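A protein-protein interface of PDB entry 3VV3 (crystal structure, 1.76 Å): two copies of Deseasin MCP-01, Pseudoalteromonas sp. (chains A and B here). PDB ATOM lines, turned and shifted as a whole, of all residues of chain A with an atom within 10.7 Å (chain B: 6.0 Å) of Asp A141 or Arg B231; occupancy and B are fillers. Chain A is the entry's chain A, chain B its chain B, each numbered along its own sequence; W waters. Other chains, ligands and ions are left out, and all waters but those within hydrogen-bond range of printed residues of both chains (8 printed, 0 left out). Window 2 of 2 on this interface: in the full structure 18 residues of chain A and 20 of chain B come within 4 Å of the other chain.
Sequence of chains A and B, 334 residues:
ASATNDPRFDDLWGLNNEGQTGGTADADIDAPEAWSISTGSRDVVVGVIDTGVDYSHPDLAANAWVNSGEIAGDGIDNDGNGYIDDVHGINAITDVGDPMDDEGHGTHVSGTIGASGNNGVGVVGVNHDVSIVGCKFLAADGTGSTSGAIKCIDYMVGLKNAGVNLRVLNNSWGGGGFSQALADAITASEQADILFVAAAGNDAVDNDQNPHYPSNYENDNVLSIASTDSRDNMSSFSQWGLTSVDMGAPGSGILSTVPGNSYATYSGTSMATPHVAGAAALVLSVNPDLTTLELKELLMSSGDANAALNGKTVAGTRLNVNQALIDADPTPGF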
ATOM      1  N   ASP A  50      -3.132 -27.487   3.489  1.00  0.00           N
ATOM      2  CA  ASP A  50      -3.032 -27.187   2.067  1.00  0.00           C
ATOM      3  C   ASP A  50      -4.226 -27.785   1.326  1.00  0.00           C
ATOM      4  O   ASP A  50      -5.336 -27.845   1.870  1.00  0.00           O
ATOM      5  CB  ASP A  50      -1.706 -27.763   1.554  1.00  0.00           C
ATOM      6  CG  ASP A  50      -1.119 -26.981   0.380  1.00  0.00           C
ATOM      7  OD1 ASP A  50      -1.752 -26.921  -0.694  1.00  0.00           O
ATOM      8  OD2 ASP A  50       0.005 -26.457   0.522  1.00  0.00           O
ATOM      9  N   THR A  51      -4.005 -28.221   0.088  1.00  0.00           N
ATOM     10  CA  THR A  51      -5.068 -28.841  -0.700  1.00  0.00           C
ATOM     11  C   THR A  51      -5.229 -30.328  -0.390  1.00  0.00           C
ATOM     12  O   THR A  51      -6.021 -31.015  -1.042  1.00  0.00           O
ATOM     13  CB  THR A  51      -4.800 -28.726  -2.218  1.00  0.00           C
ATOM     14  OG1 THR A  51      -3.618 -29.461  -2.548  1.00  0.00           O
ATOM     15  CG2 THR A  51      -4.622 -27.272  -2.638  1.00  0.00           C
ATOM     16  N   GLY A  52      -4.459 -30.822   0.576  1.00  0.00           N
ATOM     17  CA  GLY A  52      -4.480 -32.233   0.928  1.00  0.00           C
ATOM     18  C   GLY A  52      -3.121 -32.899   0.747  1.00  0.00           C
ATOM     19  O   GLY A  52      -2.122 -32.239   0.461  1.00  0.00           O
ATOM     20  N   ASN A  91     -10.370 -33.535   5.906  1.00  0.00           N
ATOM     21  CA  ASN A  91     -10.808 -32.487   4.998  1.00  0.00           C
ATOM     22  C   ASN A  91     -11.605 -31.488   5.840  1.00  0.00           C
ATOM     23  O   ASN A  91     -12.684 -31.821   6.345  1.00  0.00           O
ATOM     24  CB  ASN A  91     -11.672 -33.099   3.888  1.00  0.00           C
ATOM     25  CG  ASN A  91     -12.172 -32.071   2.881  1.00  0.00           C
ATOM     26  OD1 ASN A  91     -12.513 -30.945   3.241  1.00  0.00           O
ATOM     27  ND2 ASN A  91     -12.236 -32.469   1.610  1.00  0.00           N
ATOM     28  N   ILE A  93     -13.061 -28.811   4.937  1.00  0.00           N
ATOM     29  CA  ILE A  93     -14.219 -28.275   4.235  1.00  0.00           C
ATOM     30  C   ILE A  93     -15.461 -29.148   4.485  1.00  0.00           C
ATOM     31  O   ILE A  93     -16.549 -28.635   4.790  1.00  0.00           O
ATOM     32  CB  ILE A  93     -13.940 -28.162   2.715  1.00  0.00           C
ATOM     33  CG1 ILE A  93     -12.667 -27.347   2.459  1.00  0.00           C
ATOM     34  CG2 ILE A  93     -15.139 -27.549   2.005  1.00  0.00           C
ATOM     35  CD1 ILE A  93     -12.186 -27.418   1.011  1.00  0.00           C
ATOM     36  N   MET A 100      -7.144 -36.661   1.130  1.00  0.00           N
ATOM     37  CA  MET A 100      -6.691 -36.898  -0.245  1.00  0.00           C
ATOM     38  C   MET A 100      -6.635 -35.605  -1.066  1.00  0.00           C
ATOM     39  O   MET A 100      -7.600 -34.832  -1.128  1.00  0.00           O
ATOM     40  CB  MET A 100      -7.572 -37.934  -0.957  1.00  0.00           C
ATOM     41  CG  MET A 100      -7.251 -38.082  -2.446  1.00  0.00           C
ATOM     42  SD  MET A 100      -5.574 -38.676  -2.752  1.00  0.00           S
ATOM     43  CE  MET A 100      -5.631 -40.267  -1.942  1.00  0.00           C
ATOM     44  N   ASP A 101      -5.490 -35.393  -1.705  1.00  0.00           N
ATOM     45  CA  ASP A 101      -5.270 -34.235  -2.553  1.00  0.00           C
ATOM     46  C   ASP A 101      -5.870 -34.448  -3.942  1.00  0.00           C
ATOM     47  O   ASP A 101      -5.468 -35.363  -4.673  1.00  0.00           O
ATOM     48  CB  ASP A 101      -3.770 -34.007  -2.678  1.00  0.00           C
ATOM     49  CG  ASP A 101      -3.424 -32.740  -3.424  1.00  0.00           C
ATOM     50  OD1 ASP A 101      -4.335 -31.916  -3.684  1.00  0.00           O
ATOM     51  OD2 ASP A 101      -2.221 -32.565  -3.729  1.00  0.00           O
ATOM     52  N   ASP A 102      -6.825 -33.599  -4.302  1.00  0.00           N
ATOM     53  CA  ASP A 102      -7.437 -33.641  -5.631  1.00  0.00           C
ATOM     54  C   ASP A 102      -7.067 -32.397  -6.433  1.00  0.00           C
ATOM     55  O   ASP A 102      -7.714 -32.086  -7.434  1.00  0.00           O
ATOM     56  CB  ASP A 102      -8.961 -33.774  -5.528  1.00  0.00           C
ATOM     57  CG  ASP A 102      -9.589 -32.671  -4.695  1.00  0.00           C
ATOM     58  OD1 ASP A 102      -8.861 -31.746  -4.277  1.00  0.00           O
ATOM     59  OD2 ASP A 102     -10.814 -32.732  -4.458  1.00  0.00           O
ATOM     60  N   GLU A 103      -6.028 -31.693  -5.988  1.00  0.00           N
ATOM     61  CA  GLU A 103      -5.586 -30.461  -6.654  1.00  0.00           C
ATOM     62  C   GLU A 103      -4.143 -30.574  -7.115  1.00  0.00           C
ATOM     63  O   GLU A 103      -3.841 -30.328  -8.287  1.00  0.00           O
ATOM     64  CB  GLU A 103      -5.748 -29.255  -5.723  1.00  0.00           C
ATOM     65  CG  GLU A 103      -5.858 -27.912  -6.458  1.00  0.00           C
ATOM     66  CD  GLU A 103      -4.539 -27.437  -7.047  1.00  0.00           C
ATOM     67  OE1 GLU A 103      -3.479 -27.708  -6.447  1.00  0.00           O
ATOM     68  OE2 GLU A 103      -4.560 -26.774  -8.110  1.00  0.00           O
ATOM     69  N   GLY A 104      -3.254 -30.935  -6.191  1.00  0.00           N
ATOM     70  CA  GLY A 104      -1.847 -31.156  -6.513  1.00  0.00           C
ATOM     71  C   GLY A 104      -0.835 -30.460  -5.618  1.00  0.00           C
ATOM     72  O   GLY A 104       0.261 -30.980  -5.356  1.00  0.00           O
ATOM     73  N   HIS A 105      -1.193 -29.262  -5.162  1.00  0.00           N
ATOM     74  CA  HIS A 105      -0.267 -28.395  -4.444  1.00  0.00           C
ATOM     75  C   HIS A 105       0.231 -29.039  -3.141  1.00  0.00           C
ATOM     76  O   HIS A 105       1.431 -29.017  -2.834  1.00  0.00           O
ATOM     77  CB  HIS A 105      -0.967 -27.058  -4.167  1.00  0.00           C
ATOM     78  CG  HIS A 105      -0.061 -25.983  -3.659  1.00  0.00           C
ATOM     79  ND1 HIS A 105       0.132 -25.749  -2.313  1.00  0.00           N
ATOM     80  CD2 HIS A 105       0.692 -25.066  -4.312  1.00  0.00           C
ATOM     81  CE1 HIS A 105       0.978 -24.747  -2.156  1.00  0.00           C
ATOM     82  NE2 HIS A 105       1.333 -24.314  -3.357  1.00  0.00           N
ATOM     83  N   LYS A 136      -6.731 -30.803   4.555  1.00  0.00           N
ATOM     84  CA  LYS A 136      -7.151 -30.175   3.316  1.00  0.00           C
ATOM     85  C   LYS A 136      -8.167 -29.089   3.631  1.00  0.00           C
ATOM     86  O   LYS A 136      -9.279 -29.394   4.066  1.00  0.00           O
ATOM     87  CB  LYS A 136      -7.766 -31.244   2.402  1.00  0.00           C
ATOM     88  CG  LYS A 136      -8.436 -30.715   1.142  1.00  0.00           C
ATOM     89  CD  LYS A 136      -8.924 -31.876   0.271  1.00  0.00           C
ATOM     90  CE  LYS A 136      -9.547 -31.357  -1.020  1.00  0.00           C
ATOM     91  NZ  LYS A 136      -8.543 -30.582  -1.834  1.00  0.00           N
ATOM     92  N   PHE A 137      -7.789 -27.822   3.444  1.00  0.00           N
ATOM     93  CA  PHE A 137      -8.746 -26.723   3.597  1.00  0.00           C
ATOM     94  C   PHE A 137      -8.973 -25.986   2.273  1.00  0.00           C
ATOM     95  O   PHE A 137      -9.824 -25.104   2.194  1.00  0.00           O
ATOM     96  CB  PHE A 137      -8.343 -25.735   4.716  1.00  0.00           C
ATOM     97  CG  PHE A 137      -7.331 -24.695   4.292  1.00  0.00           C
ATOM     98  CD1 PHE A 137      -5.999 -25.038   4.099  1.00  0.00           C
ATOM     99  CD2 PHE A 137      -7.715 -23.375   4.096  1.00  0.00           C
ATOM    100  CE1 PHE A 137      -5.058 -24.080   3.712  1.00  0.00           C
ATOM    101  CE2 PHE A 137      -6.779 -22.407   3.714  1.00  0.00           C
ATOM    102  CZ  PHE A 137      -5.451 -22.764   3.521  1.00  0.00           C
ATOM    103  N   LEU A 138      -8.215 -26.365   1.245  1.00  0.00           N
ATOM    104  CA  LEU A 138      -8.384 -25.808  -0.091  1.00  0.00           C
ATOM    105  C   LEU A 138      -8.935 -26.867  -1.028  1.00  0.00           C
ATOM    106  O   LEU A 138      -8.392 -27.964  -1.117  1.00  0.00           O
ATOM    107  CB  LEU A 138      -7.045 -25.296  -0.630  1.00  0.00           C
ATOM    108  CG  LEU A 138      -6.476 -24.133   0.178  1.00  0.00           C
ATOM    109  CD1 LEU A 138      -5.035 -23.851  -0.220  1.00  0.00           C
ATOM    110  CD2 LEU A 138      -7.353 -22.890   0.018  1.00  0.00           C
ATOM    111  N   ALA A 139     -10.005 -26.523  -1.735  1.00  0.00           N
ATOM    112  CA  ALA A 139     -10.695 -27.479  -2.596  1.00  0.00           C
ATOM    113  C   ALA A 139      -9.979 -27.661  -3.923  1.00  0.00           C
ATOM    114  O   ALA A 139      -9.001 -26.963  -4.211  1.00  0.00           O
ATOM    115  CB  ALA A 139     -12.122 -27.025  -2.835  1.00  0.00           C
ATOM    116  N   ALA A 140     -10.487 -28.587  -4.734  1.00  0.00           N
ATOM    117  CA  ALA A 140      -9.919 -28.846  -6.053  1.00  0.00           C
ATOM    118  C   ALA A 140      -9.885 -27.587  -6.916  1.00  0.00           C
ATOM    119  O   ALA A 140      -9.015 -27.445  -7.790  1.00  0.00           O
ATOM    120  CB  ALA A 140     -10.699 -29.946  -6.750  1.00  0.00           C
ATOM    121  N   ASP A 141     -10.837 -26.685  -6.680  1.00  0.00           N
ATOM    122  CA  ASP A 141     -10.904 -25.435  -7.436  1.00  0.00           C
ATOM    123  C   ASP A 141     -10.343 -24.235  -6.673  1.00  0.00           C
ATOM    124  O   ASP A 141     -10.626 -23.082  -7.030  1.00  0.00           O
ATOM    125  CB  ASP A 141     -12.335 -25.141  -7.895  1.00  0.00           C
ATOM    126  CG  ASP A 141     -13.232 -24.639  -6.764  1.00  0.00           C
ATOM    127  OD1 ASP A 141     -12.850 -24.744  -5.580  1.00  0.00           O
ATOM    128  OD2 ASP A 141     -14.332 -24.129  -7.066  1.00  0.00           O
ATOM    129  N   GLY A 142      -9.571 -24.498  -5.622  1.00  0.00           N
ATOM    130  CA  GLY A 142      -8.919 -23.428  -4.881  1.00  0.00           C
ATOM    131  C   GLY A 142      -9.760 -22.783  -3.792  1.00  0.00           C
ATOM    132  O   GLY A 142      -9.275 -21.917  -3.049  1.00  0.00           O
ATOM    133  N   THR A 143     -11.016 -23.198  -3.681  1.00  0.00           N
ATOM    134  CA  THR A 143     -11.914 -22.610  -2.683  1.00  0.00           C
ATOM    135  C   THR A 143     -11.447 -22.935  -1.259  1.00  0.00           C
ATOM    136  O   THR A 143     -11.115 -24.076  -0.955  1.00  0.00           O
ATOM    137  CB  THR A 143     -13.363 -23.121  -2.857  1.00  0.00           C
ATOM    138  OG1 THR A 143     -13.844 -22.757  -4.159  1.00  0.00           O
ATOM    139  CG2 THR A 143     -14.281 -22.518  -1.788  1.00  0.00           C
ATOM    140  N   GLY A 144     -11.426 -21.927  -0.392  1.00  0.00           N
ATOM    141  CA  GLY A 144     -11.094 -22.134   1.010  1.00  0.00           C
ATOM    142  C   GLY A 144     -11.417 -20.903   1.832  1.00  0.00           C
ATOM    143  O   GLY A 144     -11.840 -19.883   1.287  1.00  0.00           O
ATOM    144  N   SER A 145     -11.224 -20.995   3.146  1.00  0.00           N
ATOM    145  CA  SER A 145     -11.526 -19.879   4.033  1.00  0.00           C
ATOM    146  C   SER A 145     -10.563 -19.838   5.203  1.00  0.00           C
ATOM    147  O   SER A 145      -9.914 -20.835   5.520  1.00  0.00           O
ATOM    148  CB  SER A 145     -12.950 -19.996   4.576  1.00  0.00           C
ATOM    149  OG  SER A 145     -13.068 -21.117   5.439  1.00  0.00           O
ATOM    150  N   TRP B  13     -16.283 -26.203 -17.034  1.00  0.00           N
ATOM    151  CA  TRP B  13     -17.463 -25.512 -16.511  1.00  0.00           C
ATOM    152  C   TRP B  13     -17.501 -24.032 -16.886  1.00  0.00           C
ATOM    153  O   TRP B  13     -18.571 -23.454 -17.026  1.00  0.00           O
ATOM    154  CB  TRP B  13     -17.565 -25.669 -14.982  1.00  0.00           C
ATOM    155  CG  TRP B  13     -16.520 -24.882 -14.237  1.00  0.00           C
ATOM    156  CD1 TRP B  13     -15.311 -25.335 -13.795  1.00  0.00           C
ATOM    157  CD2 TRP B  13     -16.590 -23.496 -13.869  1.00  0.00           C
ATOM    158  NE1 TRP B  13     -14.618 -24.315 -13.170  1.00  0.00           N
ATOM    159  CE2 TRP B  13     -15.389 -23.180 -13.196  1.00  0.00           C
ATOM    160  CE3 TRP B  13     -17.556 -22.495 -14.033  1.00  0.00           C
ATOM    161  CZ2 TRP B  13     -15.124 -21.900 -12.703  1.00  0.00           C
ATOM    162  CZ3 TRP B  13     -17.300 -21.230 -13.541  1.00  0.00           C
ATOM    163  CH2 TRP B  13     -16.087 -20.941 -12.880  1.00  0.00           C
ATOM    164  N   ASN B  17     -21.636 -24.598 -18.001  1.00  0.00           N
ATOM    165  CA  ASN B  17     -21.819 -25.139 -16.661  1.00  0.00           C
ATOM    166  C   ASN B  17     -23.258 -25.590 -16.529  1.00  0.00           C
ATOM    167  O   ASN B  17     -24.172 -24.777 -16.672  1.00  0.00           O
ATOM    168  CB  ASN B  17     -21.514 -24.042 -15.633  1.00  0.00           C
ATOM    169  CG  ASN B  17     -21.480 -24.550 -14.193  1.00  0.00           C
ATOM    170  OD1 ASN B  17     -21.874 -25.677 -13.894  1.00  0.00           O
ATOM    171  ND2 ASN B  17     -21.011 -23.697 -13.289  1.00  0.00           N
ATOM    172  N   GLY B  22     -20.193 -29.689  -9.669  1.00  0.00           N
ATOM    173  CA  GLY B  22     -20.661 -29.482  -8.308  1.00  0.00           C
ATOM    174  C   GLY B  22     -21.131 -28.066  -8.024  1.00  0.00           C
ATOM    175  O   GLY B  22     -21.497 -27.734  -6.894  1.00  0.00           O
ATOM    176  N   GLY B  23     -21.127 -27.229  -9.057  1.00  0.00           N
ATOM    177  CA  GLY B  23     -21.543 -25.849  -8.921  1.00  0.00           C
ATOM    178  C   GLY B  23     -22.964 -25.559  -9.373  1.00  0.00           C
ATOM    179  O   GLY B  23     -23.847 -26.423  -9.314  1.00  0.00           O
ATOM    180  N   THR B  24     -23.182 -24.329  -9.825  1.00  0.00           N
ATOM    181  CA  THR B  24     -24.517 -23.845 -10.166  1.00  0.00           C
ATOM    182  C   THR B  24     -24.722 -23.800 -11.669  1.00  0.00           C
ATOM    183  O   THR B  24     -23.914 -23.226 -12.395  1.00  0.00           O
ATOM    184  CB  THR B  24     -24.766 -22.443  -9.590  1.00  0.00           C
ATOM    185  OG1 THR B  24     -24.523 -22.462  -8.176  1.00  0.00           O
ATOM    186  CG2 THR B  24     -26.208 -21.996  -9.853  1.00  0.00           C
ATOM    187  N   ALA B  27     -23.627 -20.849 -14.374  1.00  0.00           N
ATOM    188  CA  ALA B  27     -22.528 -20.000 -13.929  1.00  0.00           C
ATOM    189  C   ALA B  27     -21.379 -20.255 -14.896  1.00  0.00           C
ATOM    190  O   ALA B  27     -20.519 -21.091 -14.637  1.00  0.00           O
ATOM    191  CB  ALA B  27     -22.114 -20.327 -12.489  1.00  0.00           C
ATOM    192  N   ASP B 229     -15.998 -18.501  -9.517  1.00  0.00           N
ATOM    193  CA  ASP B 229     -16.043 -19.955  -9.419  1.00  0.00           C
ATOM    194  C   ASP B 229     -17.319 -20.542 -10.007  1.00  0.00           C
ATOM    195  O   ASP B 229     -18.147 -19.828 -10.576  1.00  0.00           O
ATOM    196  CB  ASP B 229     -15.836 -20.425  -7.969  1.00  0.00           C
ATOM    197  CG  ASP B 229     -16.964 -20.005  -7.036  1.00  0.00           C
ATOM    198  OD1 ASP B 229     -18.082 -19.725  -7.511  1.00  0.00           O
ATOM    199  OD2 ASP B 229     -16.730 -19.963  -5.809  1.00  0.00           O
ATOM    200  N   SER B 230     -17.466 -21.852  -9.872  1.00  0.00           N
ATOM    201  CA  SER B 230     -18.548 -22.568 -10.538  1.00  0.00           C
ATOM    202  C   SER B 230     -19.916 -22.290  -9.928  1.00  0.00           C
ATOM    203  O   SER B 230     -20.928 -22.755 -10.461  1.00  0.00           O
ATOM    204  CB  SER B 230     -18.272 -24.068 -10.499  1.00  0.00           C
ATOM    205  OG  SER B 230     -18.301 -24.523  -9.156  1.00  0.00           O
ATOM    206  N   ARG B 231     -19.945 -21.565  -8.809  1.00  0.00           N
ATOM    207  CA  ARG B 231     -21.205 -21.117  -8.208  1.00  0.00           C
ATOM    208  C   ARG B 231     -21.462 -19.639  -8.501  1.00  0.00           C
ATOM    209  O   ARG B 231     -22.419 -19.048  -7.978  1.00  0.00           O
ATOM    210  CB  ARG B 231     -21.210 -21.328  -6.683  1.00  0.00           C
ATOM    211  CG  ARG B 231     -21.264 -22.776  -6.207  1.00  0.00           C
ATOM    212  CD  ARG B 231     -20.070 -23.061  -5.278  1.00  0.00           C
ATOM    213  NE  ARG B 231     -18.937 -23.487  -6.070  1.00  0.00           N
ATOM    214  CZ  ARG B 231     -17.653 -23.446  -5.718  1.00  0.00           C
ATOM    215  NH1 ARG B 231     -17.232 -22.993  -4.533  1.00  0.00           N
ATOM    216  NH2 ARG B 231     -16.776 -23.880  -6.594  1.00  0.00           N
ATOM    217  N   ASP B 232     -20.613 -19.049  -9.337  1.00  0.00           N
ATOM    218  CA  ASP B 232     -20.655 -17.614  -9.630  1.00  0.00           C
ATOM    219  C   ASP B 232     -20.333 -16.719  -8.416  1.00  0.00           C
ATOM    220  O   ASP B 232     -20.640 -15.527  -8.431  1.00  0.00           O
ATOM    221  CB  ASP B 232     -22.001 -17.209 -10.259  1.00  0.00           C
ATOM    222  CG  ASP B 232     -21.901 -16.926 -11.759  1.00  0.00           C
ATOM    223  OD1 ASP B 232     -20.779 -16.895 -12.318  1.00  0.00           O
ATOM    224  OD2 ASP B 232     -22.959 -16.721 -12.393  1.00  0.00           O
ATOM    225  N   ASN B 233     -19.712 -17.283  -7.377  1.00  0.00           N
ATOM    226  CA  ASN B 233     -19.108 -16.448  -6.338  1.00  0.00           C
ATOM    227  C   ASN B 233     -17.865 -15.814  -6.930  1.00  0.00           C
ATOM    228  O   ASN B 233     -17.328 -16.311  -7.921  1.00  0.00           O
ATOM    229  CB  ASN B 233     -18.608 -17.274  -5.142  1.00  0.00           C
ATOM    230  CG  ASN B 233     -19.670 -18.152  -4.525  1.00  0.00           C
ATOM    231  OD1 ASN B 233     -19.431 -19.339  -4.276  1.00  0.00           O
ATOM    232  ND2 ASN B 233     -20.837 -17.583  -4.255  1.00  0.00           N
ATOM    233  N   SER B 235     -14.153 -15.949  -6.565  1.00  0.00           N
ATOM    234  CA  SER B 235     -13.278 -16.984  -6.021  1.00  0.00           C
ATOM    235  C   SER B 235     -12.704 -16.544  -4.683  1.00  0.00           C
ATOM    236  O   SER B 235     -12.332 -15.387  -4.511  1.00  0.00           O
ATOM    237  CB  SER B 235     -12.141 -17.260  -7.012  1.00  0.00           C
ATOM    238  OG  SER B 235     -12.674 -17.612  -8.279  1.00  0.00           O
ATOM    239  N   PHE B 237      -9.980 -16.778  -3.310  1.00  0.00           N
ATOM    240  CA  PHE B 237      -8.627 -16.216  -3.390  1.00  0.00           C
ATOM    241  C   PHE B 237      -8.528 -14.900  -4.158  1.00  0.00           C
ATOM    242  O   PHE B 237      -7.481 -14.254  -4.145  1.00  0.00           O
ATOM    243  CB  PHE B 237      -7.667 -17.227  -4.030  1.00  0.00           C
ATOM    244  CG  PHE B 237      -8.127 -17.724  -5.378  1.00  0.00           C
ATOM    245  CD1 PHE B 237      -8.006 -16.924  -6.500  1.00  0.00           C
ATOM    246  CD2 PHE B 237      -8.683 -18.990  -5.514  1.00  0.00           C
ATOM    247  CE1 PHE B 237      -8.446 -17.370  -7.747  1.00  0.00           C
ATOM    248  CE2 PHE B 237      -9.124 -19.443  -6.750  1.00  0.00           C
ATOM    249  CZ  PHE B 237      -9.001 -18.631  -7.865  1.00  0.00           C
ATOM    250  N   GLY B 251     -12.084 -18.623 -12.996  1.00  0.00           N
ATOM    251  CA  GLY B 251     -10.692 -18.902 -12.687  1.00  0.00           C
ATOM    252  C   GLY B 251     -10.493 -19.987 -11.648  1.00  0.00           C
ATOM    253  O   GLY B 251      -9.357 -20.360 -11.366  1.00  0.00           O
ATOM    254  N   SER B 252     -11.581 -20.490 -11.063  1.00  0.00           N
ATOM    255  CA  SER B 252     -11.463 -21.583 -10.083  1.00  0.00           C
ATOM    256  C   SER B 252     -11.582 -22.958 -10.746  1.00  0.00           C
ATOM    257  O   SER B 252     -12.626 -23.287 -11.302  1.00  0.00           O
ATOM    258  CB  SER B 252     -12.533 -21.453  -8.996  1.00  0.00           C
ATOM    259  OG  SER B 252     -12.336 -20.268  -8.243  1.00  0.00           O
ATOM    260  N   GLY B 253     -10.523 -23.759 -10.686  1.00  0.00           N
ATOM    261  CA  GLY B 253     -10.576 -25.117 -11.206  1.00  0.00           C
ATOM    262  C   GLY B 253     -10.715 -25.173 -12.719  1.00  0.00           C
ATOM    263  O   GLY B 253     -11.654 -25.766 -13.253  1.00  0.00           O
ATOM    264  N   THR B 265      -5.448 -29.041 -14.255  1.00  0.00           N
ATOM    265  CA  THR B 265      -6.396 -28.087 -13.693  1.00  0.00           C
ATOM    266  C   THR B 265      -5.666 -27.121 -12.750  1.00  0.00           C
ATOM    267  O   THR B 265      -5.006 -27.547 -11.804  1.00  0.00           O
ATOM    268  CB  THR B 265      -7.541 -28.809 -12.961  1.00  0.00           C
ATOM    269  OG1 THR B 265      -8.233 -29.662 -13.891  1.00  0.00           O
ATOM    270  CG2 THR B 265      -8.515 -27.799 -12.358  1.00  0.00           C
ATOM    271  N   SER B 267      -5.968 -23.086 -10.677  1.00  0.00           N
ATOM    272  CA  SER B 267      -6.869 -22.034 -10.205  1.00  0.00           C
ATOM    273  C   SER B 267      -6.128 -20.722  -9.999  1.00  0.00           C
ATOM    274  O   SER B 267      -4.997 -20.703  -9.515  1.00  0.00           O
ATOM    275  CB  SER B 267      -7.518 -22.437  -8.879  1.00  0.00           C
ATOM    276  OG  SER B 267      -8.232 -23.649  -9.030  1.00  0.00           O
HETATM  277  O   HOH W   1      -3.362 -28.075  -9.870  1.00  0.00           O
HETATM  278  O   HOH W   2     -14.528 -19.796  -4.256  1.00  0.00           O
HETATM  279  O   HOH W   3      -8.971 -19.568  -1.610  1.00  0.00           O
HETATM  280  O   HOH W   4     -11.897 -20.802  -5.786  1.00  0.00           O
HETATM  281  O   HOH W   5      -7.080 -26.053  -9.195  1.00  0.00           O
HETATM  282  O   HOH W   6      -3.859 -24.272  -9.081  1.00  0.00           O
HETATM  283  O   HOH W   7      -5.492 -29.902 -10.278  1.00  0.00           O
HETATM  284  O   HOH W   8     -15.039 -23.766  -9.658  1.00  0.00           O
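Water W1 lies within hydrogen-bond range of OE2 of Glu A103 (2.5 Å) and O of Thr B265 (2.6 Å).
Water W7 bridges O of Glu A103 and O of Thr B265.
Water W5 lies within hydrogen-bond range of OG of Ser B267, O of Ala A140 and OE2 of Glu A103.
Water W8 lies within hydrogen-bond range of OD2 of Asp A141 (2.7 Å), O of Ser B252 (3.0 Å) and N of Ser B230 (3.1 Å).
Water W3 lies within hydrogen-bond range of the backbone carbonyl oxygen of Gly A142 (2.8 Å) and the backbone NH of Phe B237 (3.4 Å).
Water W6 lies within hydrogen-bond range of OE2 of Glu A103 (2.8 Å) and N of Ser B267 (2.9 Å).
Of the 21 printed residues of chain A, 4 touch a printed residue of chain B.
Among the printed residues, 9 pairs touch across the chains.
Among the printed residues, Asp or Glu carboxylates within 4 Å of a Lys or Arg side-chain nitrogen of the other chain: Asp A141 with Arg B231.
N of Glu A103 lies within hydrogen-bond range of OD1 of Asp A101 (2.9 Å).
The side-chain carboxylate (OE1) of Glu A103 is in hydrogen-bond range of the backbone NH (N) of His A105 (3.0 Å).
The side-chain hydroxyl (OG1) of Thr A143 is in hydrogen-bond range of the side-chain carboxylate (OD1) of Asp A141, at 2.6 Å.
NE1 of Trp B13 lies within hydrogen-bond range of O of Gly B253 (3.3 Å).
The side-chain hydroxyl (OG) of Ser B230 is in hydrogen-bond range of the guanidinium group (NH2) of Arg B231 (3.1 Å).
The side-chain hydroxyl of Ser B267 sits at hydrogen-bond distance from the backbone NH of Gly B253 (2.8 Å).
Among the printed residues, merely in contact across the chains: Glu A103 with Thr B265, Asp A141 with Phe B237, Asp A141 with Ser B252, Asp A141 with Gly B253, Gly A142 with Phe B237 and Gly A142 with Ser B267.
NH2 of Arg B231 is in salt-bridge range of OD2 of Asp A141 (2.5 Å).
OG of Ser B267 sits at hydrogen-bond distance from O of Asp A141.
OG1 of Thr A143 is in hydrogen-bond range of NH1 of Arg B231 (3.4 Å).
No position is printed for both chains.
Asp A50 touches none of the printed residues of chain B.
Asp A141 touches just these residues of chain B: Arg B231, Phe B237, Ser B252, Gly B253 and Ser B267.
Of the printed residues of chain B, Gly A142 touches Phe B237 (3.9 Å) and Ser B267 (3.8 Å).
No residue of chain A comes within 4 Å of Gly B23.
Thr B24 touches none of the printed residues of chain A.
No residue of chain A comes within 4 Å of Ser B230.
Arg B231 touches just these residues of chain A: Asp A141 and Thr A143.
No residue of chain A comes within 4 Å of Asp B232.
No residue of chain A comes within 4 Å of Asn B233.
Ser B235 touches none of the printed residues of chain A.
Of chain A, only Asp A141 (3.2 Å) comes within 4 Å of Ser B252.
Gly B253 touches just one residue of chain A: Asp A141.
Of the printed residues of chain A, Thr B265 touches Glu A103.
Printed residues of chain A within 4 Å of Ser B267: Asp A141 and Gly A142.
The nearest residue of chain B that does not touch Asp A141 is Asp B229 (4.1 Å).
The nearest printed residue of chain A that does not touch Thr B265 is Ala A140 (4.6 Å).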
